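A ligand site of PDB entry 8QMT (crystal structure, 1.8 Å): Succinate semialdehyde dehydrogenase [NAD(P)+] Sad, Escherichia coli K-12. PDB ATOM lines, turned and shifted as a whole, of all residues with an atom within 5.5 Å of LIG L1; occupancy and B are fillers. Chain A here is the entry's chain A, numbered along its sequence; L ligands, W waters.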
ATOM      1  N   ILE A 133      -3.393 -20.349 -12.792  1.00  0.00           N
ATOM      2  CA  ILE A 133      -2.875 -19.353 -13.723  1.00  0.00           C
ATOM      3  C   ILE A 133      -2.261 -18.237 -12.875  1.00  0.00           C
ATOM      4  O   ILE A 133      -2.987 -17.536 -12.173  1.00  0.00           O
ATOM      5  CB  ILE A 133      -3.976 -18.781 -14.638  1.00  0.00           C
ATOM      6  CG1 ILE A 133      -4.800 -19.890 -15.328  1.00  0.00           C
ATOM      7  CG2 ILE A 133      -3.384 -17.750 -15.621  1.00  0.00           C
ATOM      8  CD1 ILE A 133      -4.005 -20.807 -16.215  1.00  0.00           C
ATOM      9  N   MET A 134      -0.942 -18.074 -12.934  1.00  0.00           N
ATOM     10  CA  MET A 134      -0.244 -17.251 -11.957  1.00  0.00           C
ATOM     11  C   MET A 134       0.543 -16.122 -12.606  1.00  0.00           C
ATOM     12  O   MET A 134       0.846 -16.181 -13.809  1.00  0.00           O
ATOM     13  CB  MET A 134       0.692 -18.114 -11.100  1.00  0.00           C
ATOM     14  CG  MET A 134      -0.075 -19.069 -10.171  1.00  0.00           C
ATOM     15  SD  MET A 134      -1.026 -18.136  -8.970  1.00  0.00           S
ATOM     16  CE  MET A 134      -2.659 -18.891  -9.157  1.00  0.00           C
ATOM     17  N   PRO A 135       0.893 -15.066 -11.821  1.00  0.00           N
ATOM     18  CA  PRO A 135       1.616 -13.920 -12.373  1.00  0.00           C
ATOM     19  C   PRO A 135       3.081 -13.845 -11.958  1.00  0.00           C
ATOM     20  O   PRO A 135       3.543 -14.642 -11.135  1.00  0.00           O
ATOM     21  CB  PRO A 135       0.828 -12.741 -11.792  1.00  0.00           C
ATOM     22  CG  PRO A 135       0.547 -13.217 -10.395  1.00  0.00           C
ATOM     23  CD  PRO A 135       0.327 -14.749 -10.501  1.00  0.00           C
ATOM     24  N   TRP A 136       3.797 -12.838 -12.462  1.00  0.00           N
ATOM     25  CA  TRP A 136       5.245 -12.718 -12.315  1.00  0.00           C
ATOM     26  C   TRP A 136       5.693 -11.948 -11.078  1.00  0.00           C
ATOM     27  O   TRP A 136       6.900 -11.911 -10.804  1.00  0.00           O
ATOM     28  CB  TRP A 136       5.849 -12.018 -13.550  1.00  0.00           C
ATOM     29  CG  TRP A 136       5.072 -10.778 -13.879  1.00  0.00           C
ATOM     30  CD1 TRP A 136       4.062 -10.679 -14.801  1.00  0.00           C
ATOM     31  CD2 TRP A 136       5.156  -9.520 -13.224  1.00  0.00           C
ATOM     32  NE1 TRP A 136       3.551  -9.397 -14.787  1.00  0.00           N
ATOM     33  CE2 TRP A 136       4.196  -8.674 -13.822  1.00  0.00           C
ATOM     34  CE3 TRP A 136       5.973  -8.995 -12.206  1.00  0.00           C
ATOM     35  CZ2 TRP A 136       4.019  -7.338 -13.429  1.00  0.00           C
ATOM     36  CZ3 TRP A 136       5.797  -7.673 -11.813  1.00  0.00           C
ATOM     37  CH2 TRP A 136       4.832  -6.861 -12.426  1.00  0.00           C
ATOM     38  N   ASN A 137       4.802 -11.292 -10.331  1.00  0.00           N
ATOM     39  CA  ASN A 137       5.295 -10.366  -9.307  1.00  0.00           C
ATOM     40  C   ASN A 137       5.832 -11.064  -8.068  1.00  0.00           C
ATOM     41  O   ASN A 137       6.791 -10.569  -7.456  1.00  0.00           O
ATOM     42  CB  ASN A 137       4.208  -9.340  -8.952  1.00  0.00           C
ATOM     43  CG  ASN A 137       2.994  -9.947  -8.262  1.00  0.00           C
ATOM     44  OD1 ASN A 137       2.635 -11.113  -8.464  1.00  0.00           O
ATOM     45  ND2 ASN A 137       2.341  -9.126  -7.444  1.00  0.00           N
ATOM     46  N   GLN A 142       3.339 -16.763  -5.105  1.00  0.00           N
ATOM     47  CA  GLN A 142       2.009 -16.923  -5.710  1.00  0.00           C
ATOM     48  C   GLN A 142       1.668 -18.390  -5.949  1.00  0.00           C
ATOM     49  O   GLN A 142       0.524 -18.838  -5.733  1.00  0.00           O
ATOM     50  CB  GLN A 142       1.922 -16.153  -7.034  1.00  0.00           C
ATOM     51  CG  GLN A 142       2.045 -14.637  -6.946  1.00  0.00           C
ATOM     52  CD  GLN A 142       0.725 -13.974  -6.669  1.00  0.00           C
ATOM     53  OE1 GLN A 142      -0.229 -14.633  -6.249  1.00  0.00           O
ATOM     54  NE2 GLN A 142       0.650 -12.660  -6.925  1.00  0.00           N
ATOM     55  N   LYS A 160       0.147 -22.962 -14.814  1.00  0.00           N
ATOM     56  CA  LYS A 160       0.443 -22.197 -16.022  1.00  0.00           C
ATOM     57  C   LYS A 160       1.004 -20.867 -15.520  1.00  0.00           C
ATOM     58  O   LYS A 160       0.253 -20.012 -15.037  1.00  0.00           O
ATOM     59  CB  LYS A 160      -0.815 -22.026 -16.884  1.00  0.00           C
ATOM     60  CG  LYS A 160      -0.554 -21.847 -18.380  1.00  0.00           C
ATOM     61  CD  LYS A 160       0.285 -20.611 -18.704  1.00  0.00           C
ATOM     62  CE  LYS A 160      -0.465 -19.298 -18.410  1.00  0.00           C
ATOM     63  NZ  LYS A 160       0.385 -18.150 -18.852  1.00  0.00           N
ATOM     64  N   HIS A 161       2.316 -20.710 -15.590  1.00  0.00           N
ATOM     65  CA  HIS A 161       2.956 -19.516 -15.046  1.00  0.00           C
ATOM     66  C   HIS A 161       3.054 -18.410 -16.095  1.00  0.00           C
ATOM     67  O   HIS A 161       2.850 -18.629 -17.285  1.00  0.00           O
ATOM     68  CB  HIS A 161       4.339 -19.868 -14.494  1.00  0.00           C
ATOM     69  CG  HIS A 161       4.680 -19.139 -13.237  1.00  0.00           C
ATOM     70  ND1 HIS A 161       4.099 -17.939 -12.893  1.00  0.00           N
ATOM     71  CD2 HIS A 161       5.528 -19.457 -12.235  1.00  0.00           C
ATOM     72  CE1 HIS A 161       4.584 -17.537 -11.737  1.00  0.00           C
ATOM     73  NE2 HIS A 161       5.466 -18.434 -11.319  1.00  0.00           N
ATOM     74  N   ALA A 162       3.350 -17.186 -15.610  1.00  0.00           N
ATOM     75  CA  ALA A 162       3.492 -16.037 -16.491  1.00  0.00           C
ATOM     76  C   ALA A 162       4.662 -16.260 -17.441  1.00  0.00           C
ATOM     77  O   ALA A 162       5.679 -16.837 -17.055  1.00  0.00           O
ATOM     78  CB  ALA A 162       3.720 -14.746 -15.672  1.00  0.00           C
ATOM     79  N   PRO A 163       4.552 -15.823 -18.706  1.00  0.00           N
ATOM     80  CA  PRO A 163       5.546 -16.218 -19.714  1.00  0.00           C
ATOM     81  C   PRO A 163       6.919 -15.593 -19.516  1.00  0.00           C
ATOM     82  O   PRO A 163       7.870 -16.027 -20.188  1.00  0.00           O
ATOM     83  CB  PRO A 163       4.914 -15.751 -21.031  1.00  0.00           C
ATOM     84  CG  PRO A 163       3.943 -14.675 -20.633  1.00  0.00           C
ATOM     85  CD  PRO A 163       3.409 -15.098 -19.288  1.00  0.00           C
ATOM     86  N   ASP A 192      -0.098 -21.585 -24.032  1.00  0.00           N
ATOM     87  CA  ASP A 192      -0.605 -20.276 -24.397  1.00  0.00           C
ATOM     88  C   ASP A 192      -2.062 -20.185 -23.971  1.00  0.00           C
ATOM     89  O   ASP A 192      -2.605 -21.099 -23.336  1.00  0.00           O
ATOM     90  CB  ASP A 192      -0.383 -20.006 -25.887  1.00  0.00           C
ATOM     91  CG  ASP A 192      -1.103 -21.000 -26.791  1.00  0.00           C
ATOM     92  OD1 ASP A 192      -1.901 -21.830 -26.306  1.00  0.00           O
ATOM     93  OD2 ASP A 192      -0.851 -20.952 -28.018  1.00  0.00           O
ATOM     94  N   ASN A 193      -2.716 -19.063 -24.283  1.00  0.00           N
ATOM     95  CA  ASN A 193      -4.073 -18.839 -23.808  1.00  0.00           C
ATOM     96  C   ASN A 193      -5.035 -19.892 -24.371  1.00  0.00           C
ATOM     97  O   ASN A 193      -5.915 -20.363 -23.647  1.00  0.00           O
ATOM     98  CB  ASN A 193      -4.532 -17.435 -24.181  1.00  0.00           C
ATOM     99  CG  ASN A 193      -3.875 -16.360 -23.334  1.00  0.00           C
ATOM    100  OD1 ASN A 193      -2.970 -16.656 -22.557  1.00  0.00           O
ATOM    101  ND2 ASN A 193      -4.324 -15.112 -23.480  1.00  0.00           N
ATOM    102  N   VAL A 196      -4.712 -22.998 -22.352  1.00  0.00           N
ATOM    103  CA  VAL A 196      -5.495 -22.850 -21.121  1.00  0.00           C
ATOM    104  C   VAL A 196      -6.972 -23.101 -21.402  1.00  0.00           C
ATOM    105  O   VAL A 196      -7.665 -23.783 -20.635  1.00  0.00           O
ATOM    106  CB  VAL A 196      -5.263 -21.464 -20.495  1.00  0.00           C
ATOM    107  CG1 VAL A 196      -6.247 -21.207 -19.378  1.00  0.00           C
ATOM    108  CG2 VAL A 196      -3.812 -21.348 -19.987  1.00  0.00           C
ATOM    109  N   VAL A 210      -6.928 -18.222 -10.352  1.00  0.00           N
ATOM    110  CA  VAL A 210      -6.319 -17.190 -11.172  1.00  0.00           C
ATOM    111  C   VAL A 210      -5.836 -16.054 -10.281  1.00  0.00           C
ATOM    112  O   VAL A 210      -6.613 -15.511  -9.497  1.00  0.00           O
ATOM    113  CB  VAL A 210      -7.283 -16.615 -12.229  1.00  0.00           C
ATOM    114  CG1 VAL A 210      -6.586 -15.591 -13.085  1.00  0.00           C
ATOM    115  CG2 VAL A 210      -7.876 -17.737 -13.076  1.00  0.00           C
ATOM    116  N   THR A 211      -4.560 -15.686 -10.425  1.00  0.00           N
ATOM    117  CA  THR A 211      -4.036 -14.440  -9.863  1.00  0.00           C
ATOM    118  C   THR A 211      -3.442 -13.622 -10.996  1.00  0.00           C
ATOM    119  O   THR A 211      -2.518 -14.084 -11.683  1.00  0.00           O
ATOM    120  CB  THR A 211      -2.989 -14.709  -8.782  1.00  0.00           C
ATOM    121  OG1 THR A 211      -3.602 -15.458  -7.714  1.00  0.00           O
ATOM    122  CG2 THR A 211      -2.444 -13.382  -8.252  1.00  0.00           C
ATOM    123  N   GLY A 212      -4.003 -12.447 -11.237  1.00  0.00           N
ATOM    124  CA  GLY A 212      -3.513 -11.609 -12.315  1.00  0.00           C
ATOM    125  C   GLY A 212      -4.341 -10.368 -12.516  1.00  0.00           C
ATOM    126  O   GLY A 212      -4.841  -9.797 -11.550  1.00  0.00           O
ATOM    127  N   SER A 213      -4.495  -9.934 -13.764  1.00  0.00           N
ATOM    128  CA  SER A 213      -5.204  -8.711 -14.040  1.00  0.00           C
ATOM    129  C   SER A 213      -6.707  -8.952 -14.040  1.00  0.00           C
ATOM    130  O   SER A 213      -7.188 -10.075 -14.135  1.00  0.00           O
ATOM    131  CB  SER A 213      -4.780  -8.127 -15.397  1.00  0.00           C
ATOM    132  OG  SER A 213      -5.131  -9.002 -16.457  1.00  0.00           O
ATOM    133  N   VAL A 214      -7.453  -7.849 -13.947  1.00  0.00           N
ATOM    134  CA  VAL A 214      -8.904  -7.901 -14.057  1.00  0.00           C
ATOM    135  C   VAL A 214      -9.307  -8.504 -15.397  1.00  0.00           C
ATOM    136  O   VAL A 214     -10.216  -9.352 -15.465  1.00  0.00           O
ATOM    137  CB  VAL A 214      -9.480  -6.489 -13.864  1.00  0.00           C
ATOM    138  CG1 VAL A 214     -10.927  -6.441 -14.296  1.00  0.00           C
ATOM    139  CG2 VAL A 214      -9.335  -6.060 -12.416  1.00  0.00           C
ATOM    140  N   ALA A 216      -7.648 -10.640 -17.257  1.00  0.00           N
ATOM    141  CA  ALA A 216      -7.397 -12.081 -17.253  1.00  0.00           C
ATOM    142  C   ALA A 216      -8.460 -12.822 -16.445  1.00  0.00           C
ATOM    143  O   ALA A 216      -8.955 -13.880 -16.867  1.00  0.00           O
ATOM    144  CB  ALA A 216      -6.004 -12.351 -16.663  1.00  0.00           C
ATOM    145  N   ALA A 219     -11.682 -13.005 -18.515  1.00  0.00           N
ATOM    146  CA  ALA A 219     -11.588 -13.961 -19.613  1.00  0.00           C
ATOM    147  C   ALA A 219     -11.591 -15.391 -19.112  1.00  0.00           C
ATOM    148  O   ALA A 219     -12.266 -16.258 -19.679  1.00  0.00           O
ATOM    149  CB  ALA A 219     -10.333 -13.702 -20.443  1.00  0.00           C
ATOM    150  N   ILE A 220     -10.840 -15.682 -18.053  1.00  0.00           N
ATOM    151  CA  ILE A 220     -10.757 -17.051 -17.570  1.00  0.00           C
ATOM    152  C   ILE A 220     -12.007 -17.420 -16.780  1.00  0.00           C
ATOM    153  O   ILE A 220     -12.554 -18.525 -16.938  1.00  0.00           O
ATOM    154  CB  ILE A 220      -9.470 -17.234 -16.727  1.00  0.00           C
ATOM    155  CG1 ILE A 220      -8.230 -17.063 -17.616  1.00  0.00           C
ATOM    156  CG2 ILE A 220      -9.448 -18.598 -16.087  1.00  0.00           C
ATOM    157  CD1 ILE A 220      -6.957 -16.777 -16.852  1.00  0.00           C
ATOM    158  N   GLN A 223     -14.765 -18.510 -18.944  1.00  0.00           N
ATOM    159  CA  GLN A 223     -14.585 -19.854 -19.489  1.00  0.00           C
ATOM    160  C   GLN A 223     -14.827 -20.924 -18.426  1.00  0.00           C
ATOM    161  O   GLN A 223     -15.395 -21.989 -18.722  1.00  0.00           O
ATOM    162  CB  GLN A 223     -13.181 -19.997 -20.064  1.00  0.00           C
ATOM    163  CG  GLN A 223     -12.883 -19.099 -21.250  1.00  0.00           C
ATOM    164  CD  GLN A 223     -11.449 -19.271 -21.725  1.00  0.00           C
ATOM    165  OE1 GLN A 223     -11.099 -20.303 -22.290  1.00  0.00           O
ATOM    166  NE2 GLN A 223     -10.615 -18.287 -21.459  1.00  0.00           N
ATOM    167  N   GLU A 234      -8.139 -13.681  -7.898  1.00  0.00           N
ATOM    168  CA  GLU A 234      -7.506 -12.571  -7.130  1.00  0.00           C
ATOM    169  C   GLU A 234      -6.933 -11.646  -8.205  1.00  0.00           C
ATOM    170  O   GLU A 234      -5.925 -12.005  -8.806  1.00  0.00           O
ATOM    171  CB  GLU A 234      -6.491 -13.078  -6.104  1.00  0.00           C
ATOM    172  CG  GLU A 234      -6.024 -11.974  -5.176  1.00  0.00           C
ATOM    173  CD  GLU A 234      -4.819 -11.205  -5.691  1.00  0.00           C
ATOM    174  OE1 GLU A 234      -3.714 -11.768  -5.660  1.00  0.00           O
ATOM    175  OE2 GLU A 234      -5.003 -10.063  -6.141  1.00  0.00           O
ATOM    176  N   LEU A 235      -7.539 -10.475  -8.408  1.00  0.00           N
ATOM    177  CA  LEU A 235      -7.203  -9.667  -9.610  1.00  0.00           C
ATOM    178  C   LEU A 235      -6.644  -8.276  -9.304  1.00  0.00           C
ATOM    179  O   LEU A 235      -6.848  -7.365 -10.109  1.00  0.00           O
ATOM    180  CB  LEU A 235      -8.496  -9.593 -10.433  1.00  0.00           C
ATOM    181  CG  LEU A 235      -9.204 -10.926 -10.642  1.00  0.00           C
ATOM    182  CD1 LEU A 235     -10.473 -10.738 -11.453  1.00  0.00           C
ATOM    183  CD2 LEU A 235      -8.274 -11.922 -11.307  1.00  0.00           C
ATOM    184  N   GLY A 236      -5.913  -8.151  -8.218  1.00  0.00           N
ATOM    185  CA  GLY A 236      -5.272  -6.891  -7.929  1.00  0.00           C
ATOM    186  C   GLY A 236      -6.147  -5.987  -7.097  1.00  0.00           C
ATOM    187  O   GLY A 236      -7.252  -6.324  -6.678  1.00  0.00           O
ATOM    188  N   VAL A 267       2.576  -4.976  -6.190  1.00  0.00           N
ATOM    189  CA  VAL A 267       1.890  -5.845  -5.239  1.00  0.00           C
ATOM    190  C   VAL A 267       0.394  -5.609  -5.335  1.00  0.00           C
ATOM    191  O   VAL A 267      -0.064  -4.461  -5.309  1.00  0.00           O
ATOM    192  CB  VAL A 267       2.381  -5.604  -3.795  1.00  0.00           C
ATOM    193  CG1 VAL A 267       1.771  -6.654  -2.855  1.00  0.00           C
ATOM    194  CG2 VAL A 267       3.915  -5.638  -3.718  1.00  0.00           C
ATOM    195  N   CYS A 268      -0.387  -6.686  -5.415  1.00  0.00           N
ATOM    196  CA  CYS A 268      -1.873  -6.557  -5.501  1.00  0.00           C
ATOM    197  C   CYS A 268      -2.381  -5.766  -4.294  1.00  0.00           C
ATOM    198  O   CYS A 268      -3.264  -4.935  -4.466  1.00  0.00           O
ATOM    199  CB  CYS A 268      -2.496  -7.936  -5.488  1.00  0.00           C
ATOM    200  SG  CYS A 268      -1.886  -8.981  -4.146  1.00  0.00           S
ATOM    201  N   ARG A 312       8.375  -5.396 -16.416  1.00  0.00           N
ATOM    202  CA  ARG A 312       8.026  -5.458 -17.833  1.00  0.00           C
ATOM    203  C   ARG A 312       8.139  -4.083 -18.463  1.00  0.00           C
ATOM    204  O   ARG A 312       7.573  -3.119 -17.939  1.00  0.00           O
ATOM    205  CB  ARG A 312       6.616  -6.020 -18.028  1.00  0.00           C
ATOM    206  CG  ARG A 312       6.493  -7.501 -17.720  1.00  0.00           C
ATOM    207  CD  ARG A 312       6.102  -8.283 -18.955  1.00  0.00           C
ATOM    208  NE  ARG A 312       4.906  -7.687 -19.542  1.00  0.00           N
ATOM    209  CZ  ARG A 312       3.667  -8.034 -19.222  1.00  0.00           C
ATOM    210  NH1 ARG A 312       3.425  -9.041 -18.385  1.00  0.00           N
ATOM    211  NH2 ARG A 312       2.657  -7.360 -19.750  1.00  0.00           N
ATOM    212  N   LEU A 315       4.884  -2.518 -19.287  1.00  0.00           N
ATOM    213  CA  LEU A 315       4.133  -2.087 -18.119  1.00  0.00           C
ATOM    214  C   LEU A 315       4.709  -0.817 -17.501  1.00  0.00           C
ATOM    215  O   LEU A 315       3.954  -0.027 -16.924  1.00  0.00           O
ATOM    216  CB  LEU A 315       4.065  -3.220 -17.091  1.00  0.00           C
ATOM    217  CG  LEU A 315       3.281  -4.453 -17.568  1.00  0.00           C
ATOM    218  CD1 LEU A 315       3.229  -5.526 -16.483  1.00  0.00           C
ATOM    219  CD2 LEU A 315       1.870  -4.074 -18.039  1.00  0.00           C
ATOM    220  N   GLU A 318       3.013   1.675 -19.607  1.00  0.00           N
ATOM    221  CA  GLU A 318       1.598   1.840 -19.201  1.00  0.00           C
ATOM    222  C   GLU A 318       1.531   2.704 -17.938  1.00  0.00           C
ATOM    223  O   GLU A 318       0.716   3.617 -17.887  1.00  0.00           O
ATOM    224  CB  GLU A 318       0.962   0.458 -18.998  1.00  0.00           C
ATOM    225  CG  GLU A 318      -0.421   0.492 -18.381  1.00  0.00           C
ATOM    226  CD  GLU A 318      -1.024  -0.898 -18.237  1.00  0.00           C
ATOM    227  OE1 GLU A 318      -1.199  -1.572 -19.257  1.00  0.00           O
ATOM    228  OE2 GLU A 318      -1.312  -1.289 -17.084  1.00  0.00           O
ATOM    229  N   GLU A 365      -5.618   0.596 -11.134  1.00  0.00           N
ATOM    230  CA  GLU A 365      -4.506   0.038 -10.368  1.00  0.00           C
ATOM    231  C   GLU A 365      -3.190   0.619 -10.882  1.00  0.00           C
ATOM    232  O   GLU A 365      -2.901   0.529 -12.069  1.00  0.00           O
ATOM    233  CB  GLU A 365      -4.488  -1.488 -10.448  1.00  0.00           C
ATOM    234  CG  GLU A 365      -3.315  -2.083  -9.641  1.00  0.00           C
ATOM    235  CD  GLU A 365      -3.374  -3.595  -9.522  1.00  0.00           C
ATOM    236  OE1 GLU A 365      -3.714  -4.256 -10.512  1.00  0.00           O
ATOM    237  OE2 GLU A 365      -3.052  -4.124  -8.423  1.00  0.00           O
ATOM    238  N   PHE A 367       0.321  -0.087 -10.828  1.00  0.00           N
ATOM    239  CA  PHE A 367       1.115  -1.265 -10.462  1.00  0.00           C
ATOM    240  C   PHE A 367       2.615  -0.995 -10.621  1.00  0.00           C
ATOM    241  O   PHE A 367       3.336  -1.642 -11.378  1.00  0.00           O
ATOM    242  CB  PHE A 367       0.687  -2.476 -11.296  1.00  0.00           C
ATOM    243  CG  PHE A 367       0.822  -3.794 -10.574  1.00  0.00           C
ATOM    244  CD1 PHE A 367       0.012  -4.082  -9.486  1.00  0.00           C
ATOM    245  CD2 PHE A 367       1.762  -4.742 -10.982  1.00  0.00           C
ATOM    246  CE1 PHE A 367       0.126  -5.305  -8.807  1.00  0.00           C
ATOM    247  CE2 PHE A 367       1.864  -5.963 -10.323  1.00  0.00           C
ATOM    248  CZ  PHE A 367       1.060  -6.244  -9.235  1.00  0.00           C
HETATM  249  P1  LIG L   1      -1.861 -10.728 -16.835  1.00  0.00           P
HETATM  250  O1  LIG L   1      -3.186 -10.953 -16.238  1.00  0.00           O
HETATM  251  O2  LIG L   1      -2.027 -10.577 -18.412  1.00  0.00           O
HETATM  252  O3  LIG L   1      -0.890 -11.980 -16.534  1.00  0.00           O
HETATM  253  C1  LIG L   1      -1.423 -12.761 -15.474  1.00  0.00           C
HETATM  254  C2  LIG L   1      -1.377 -14.267 -15.771  1.00  0.00           C
HETATM  255  O4  LIG L   1      -2.582 -14.644 -16.449  1.00  0.00           O
HETATM  256  C3  LIG L   1      -0.232 -14.678 -16.700  1.00  0.00           C
HETATM  257  O5  LIG L   1       0.163 -16.016 -16.446  1.00  0.00           O
HETATM  258  C4  LIG L   1      -0.883 -14.609 -18.095  1.00  0.00           C
HETATM  259  O6  LIG L   1      -0.188 -15.456 -19.003  1.00  0.00           O
HETATM  260  C5  LIG L   1      -2.252 -15.213 -17.738  1.00  0.00           C
HETATM  261  N1  LIG L   1      -3.328 -14.832 -18.649  1.00  0.00           N
HETATM  262  C6  LIG L   1      -3.752 -13.583 -18.954  1.00  0.00           C
HETATM  263  N2  LIG L   1      -4.758 -13.642 -19.770  1.00  0.00           N
HETATM  264  C7  LIG L   1      -5.046 -14.935 -20.029  1.00  0.00           C
HETATM  265  C8  LIG L   1      -5.989 -15.600 -20.806  1.00  0.00           C
HETATM  266  N3  LIG L   1      -6.915 -14.889 -21.546  1.00  0.00           N
HETATM  267  N4  LIG L   1      -5.980 -16.919 -20.827  1.00  0.00           N
HETATM  268  C9  LIG L   1      -5.109 -17.599 -20.128  1.00  0.00           C
HETATM  269  N5  LIG L   1      -4.204 -17.034 -19.372  1.00  0.00           N
HETATM  270  C10 LIG L   1      -4.138 -15.709 -19.306  1.00  0.00           C
HETATM  271  O7  LIG L   1      -1.325  -9.369 -16.181  1.00  0.00           O
HETATM  272  P2  LIG L   1       0.078  -8.784 -16.719  1.00  0.00           P
HETATM  273  O8  LIG L   1       0.044  -8.437 -18.219  1.00  0.00           O
HETATM  274  O9  LIG L   1       1.247  -9.724 -16.427  1.00  0.00           O
HETATM  275  O10 LIG L   1       0.304  -7.439 -15.876  1.00  0.00           O
HETATM  276  C11 LIG L   1      -0.722  -6.521 -16.271  1.00  0.00           C
HETATM  277  C12 LIG L   1      -1.431  -5.915 -15.064  1.00  0.00           C
HETATM  278  O11 LIG L   1      -2.161  -6.942 -14.341  1.00  0.00           O
HETATM  279  C13 LIG L   1      -0.424  -5.378 -14.022  1.00  0.00           C
HETATM  280  O12 LIG L   1       0.052  -4.075 -14.354  1.00  0.00           O
HETATM  281  C14 LIG L   1      -1.339  -5.343 -12.781  1.00  0.00           C
HETATM  282  O13 LIG L   1      -2.211  -4.211 -12.814  1.00  0.00           O
HETATM  283  C15 LIG L   1      -2.145  -6.650 -12.924  1.00  0.00           C
HETATM  284  N6  LIG L   1      -1.486  -7.718 -12.185  1.00  0.00           N
HETATM  285  C16 LIG L   1      -2.000  -8.115 -11.037  1.00  0.00           C
HETATM  286  C17 LIG L   1      -1.370  -9.125 -10.314  1.00  0.00           C
HETATM  287  C18 LIG L   1      -1.912  -9.600  -9.035  1.00  0.00           C
HETATM  288  O14 LIG L   1      -1.145  -9.972  -8.174  1.00  0.00           O
HETATM  289  N7  LIG L   1      -3.237  -9.641  -8.824  1.00  0.00           N
HETATM  290  C19 LIG L   1      -0.207  -9.703 -10.805  1.00  0.00           C
HETATM  291  C20 LIG L   1       0.295  -9.258 -12.009  1.00  0.00           C
HETATM  292  C21 LIG L   1      -0.389  -8.263 -12.666  1.00  0.00           C
HETATM  293  C1  LG2 L   2       0.408 -11.852  -1.714  1.00  0.00           C
HETATM  294  O1  LG2 L   2       1.189 -11.657  -0.759  1.00  0.00           O
HETATM  295  C2  LG2 L   2       0.091 -10.666  -2.622  1.00  0.00           C
HETATM  296  O2  LG2 L   2      -0.102 -12.991  -1.883  1.00  0.00           O
HETATM  297  C3  LG2 L   2      -0.284 -11.091  -4.034  1.00  0.00           C
HETATM  298  C4  LG2 L   2      -0.592  -9.810  -4.801  1.00  0.00           C
HETATM  299  O3  LG2 L   2       0.179  -9.381  -5.577  1.00  0.00           O
HETATM  300  O   HOH W   1       0.067 -11.528 -19.932  1.00  0.00           O
HETATM  301  O   HOH W   2      -2.628  -1.470 -14.138  1.00  0.00           O
HETATM  302  O   HOH W   3      -7.848 -18.629 -22.084  1.00  0.00           O
HETATM  303  O   HOH W   4      -7.368 -11.809 -22.147  1.00  0.00           O
HETATM  304  O   HOH W   5      -3.685  -9.634 -19.943  1.00  0.00           O
HETATM  305  O   HOH W   6      -1.031 -15.115 -21.443  1.00  0.00           O
HETATM  306  O   HOH W   7       1.855 -12.187 -17.722  1.00  0.00           O
HETATM  307  O   HOH W   8       3.361  -3.124 -13.757  1.00  0.00           O
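O5 of LIG L1 lies within hydrogen-bond range of O of Met 134 (2.7 Å).
The side-chain carboxylate (OE1) of Glu 365 lies within hydrogen-bond range of an oxygen (O13) of LIG L1 (2.7 Å).
An oxygen (O6) of LIG L1 sits at hydrogen-bond distance from the side-chain amino group (NZ) of Lys 160 (2.8 Å).
The backbone NH of Ser 213 is in hydrogen-bond range of an oxygen (O1) of LIG L1, at 3.0 Å.
An oxygen (O1) of LIG L1 lies within hydrogen-bond range of the side-chain hydroxyl (OG) of Ser 213, 2.8 Å away.
O9 of LIG L1 is in hydrogen-bond range of NE1 of Trp 136 (2.8 Å).
The guanidinium group of Arg 312 lies within salt-bridge range of an oxygen (O9) of LIG L1, at 3.0 Å.
O of Gly 212 lies within hydrogen-bond range of N7 of LIG L1, at 3.2 Å.
ND2 of Asn 193 lies close to N3 of LIG L1 (3.2 Å).
N7 of LIG L1 sits at hydrogen-bond distance from OE2 of Glu 234 (3.2 Å).
O5 of LIG L1 lies close to N of Ala 162, at 3.5 Å.
The side-chain amide nitrogen (NE2) of Gln 142 sits at hydrogen-bond distance from an oxygen (O14) of LIG L1 (3.5 Å).
O3 of LG2 L2 is in hydrogen-bond range of N of Cys 268 (2.8 Å).
SG of Cys 268 is covalently linked to C4 of LG2 L2 (1.7 Å).
ND2 of Asn 137 is in hydrogen-bond range of O3 of LG2 L2 (2.9 Å).
The backbone carbonyl oxygen (O) of Met 134 sits at hydrogen-bond distance from the backbone NH (N) of Ala 162 (3.2 Å).
The side-chain hydroxyl (OG) of Ser 213 sits at hydrogen-bond distance from the backbone NH (N) of Ala 216.
The backbone NH of Gly 236 lies within hydrogen-bond range of the side-chain carboxylate of Glu 234.
The backbone carbonyl oxygen (O) of Glu 234 is in hydrogen-bond range of the backbone NH (N) of Gly 212, at 3.1 Å.
The backbone NH (N) of Glu 234 lies within hydrogen-bond range of the backbone carbonyl oxygen (O) of Val 210.
The backbone NH of Thr 211 is in hydrogen-bond range of the backbone carbonyl oxygen of Ile 133, 3.0 Å away.
The side-chain amide oxygen (OD1) of Asn 137 lies within hydrogen-bond range of the side-chain amide nitrogen (NE2) of Gln 142 (2.9 Å).
The side-chain amide nitrogen of Gln 223 sits at hydrogen-bond distance from the backbone carbonyl oxygen of Ala 219 (3.2 Å).
The backbone NH of Gly 236 lies close to a nitrogen (N7) of LIG L1 (3.1 Å).
Merely in contact with LIG L1: Ala 216 (3.2 Å), Ile 133 (3.3 Å), Pro 135 (3.4 Å), Phe 367 (3.5 Å), Leu 315 (3.5 Å), Pro 163 (3.6 Å), Cys 268 (3.6 Å), Thr 211 (3.6 Å), Asn 137 (3.7 Å), Leu 235 (3.7 Å), Ile 220 (3.7 Å), His 161 (3.8 Å), Ala 219 (3.8 Å) and Val 196 (3.9 Å).
Hydrophobic or aromatic side chains within 4 Å of LIG L1: Ile 133, Pro 135, Trp 136, Ala 162, Pro 163, Val 196, Ala 216, Ala 219, Ile 220, Leu 315 and Phe 367.
26 residues have an atom within 4 Å of LIG L1: Ile 133, Met 134, Pro 135, Trp 136, Asn 137, Gln 142, Lys 160, His 161, Ala 162, Pro 163, Asn 193, Val 196, Thr 211, Gly 212, Ser 213, Ala 216, Ala 219, Ile 220, Glu 234, Leu 235, Gly 236, Cys 268, Arg 312, Leu 315, Glu 365 and Phe 367.
Along chain A the residues within 4 Å of LIG L1 span positions 133 to 367.
The nearest printed residue that does not touch LIG L1 is Glu 318 (4.1 Å).
Water W6 bridges an oxygen (O6) of LIG L1 (2.6 Å) and the side-chain amide oxygen of Asn 193 (2.7 Å).
Water W3 lies within hydrogen-bond range of a nitrogen (N4) of LIG L1, the side-chain amide nitrogen (NE2) of Gln 223 and the backbone carbonyl oxygen (O) of Asn 193.
Water W2 lies within hydrogen-bond range of O of Glu 365 (2.9 Å), O13 of LIG L1 (3.1 Å) and OE2 of Glu 318 (3.2 Å).
Water W8 lies within hydrogen-bond range of the backbone carbonyl oxygen (O) of Phe 367 (2.8 Å) and an oxygen (O12) of LIG L1 (3.5 Å).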
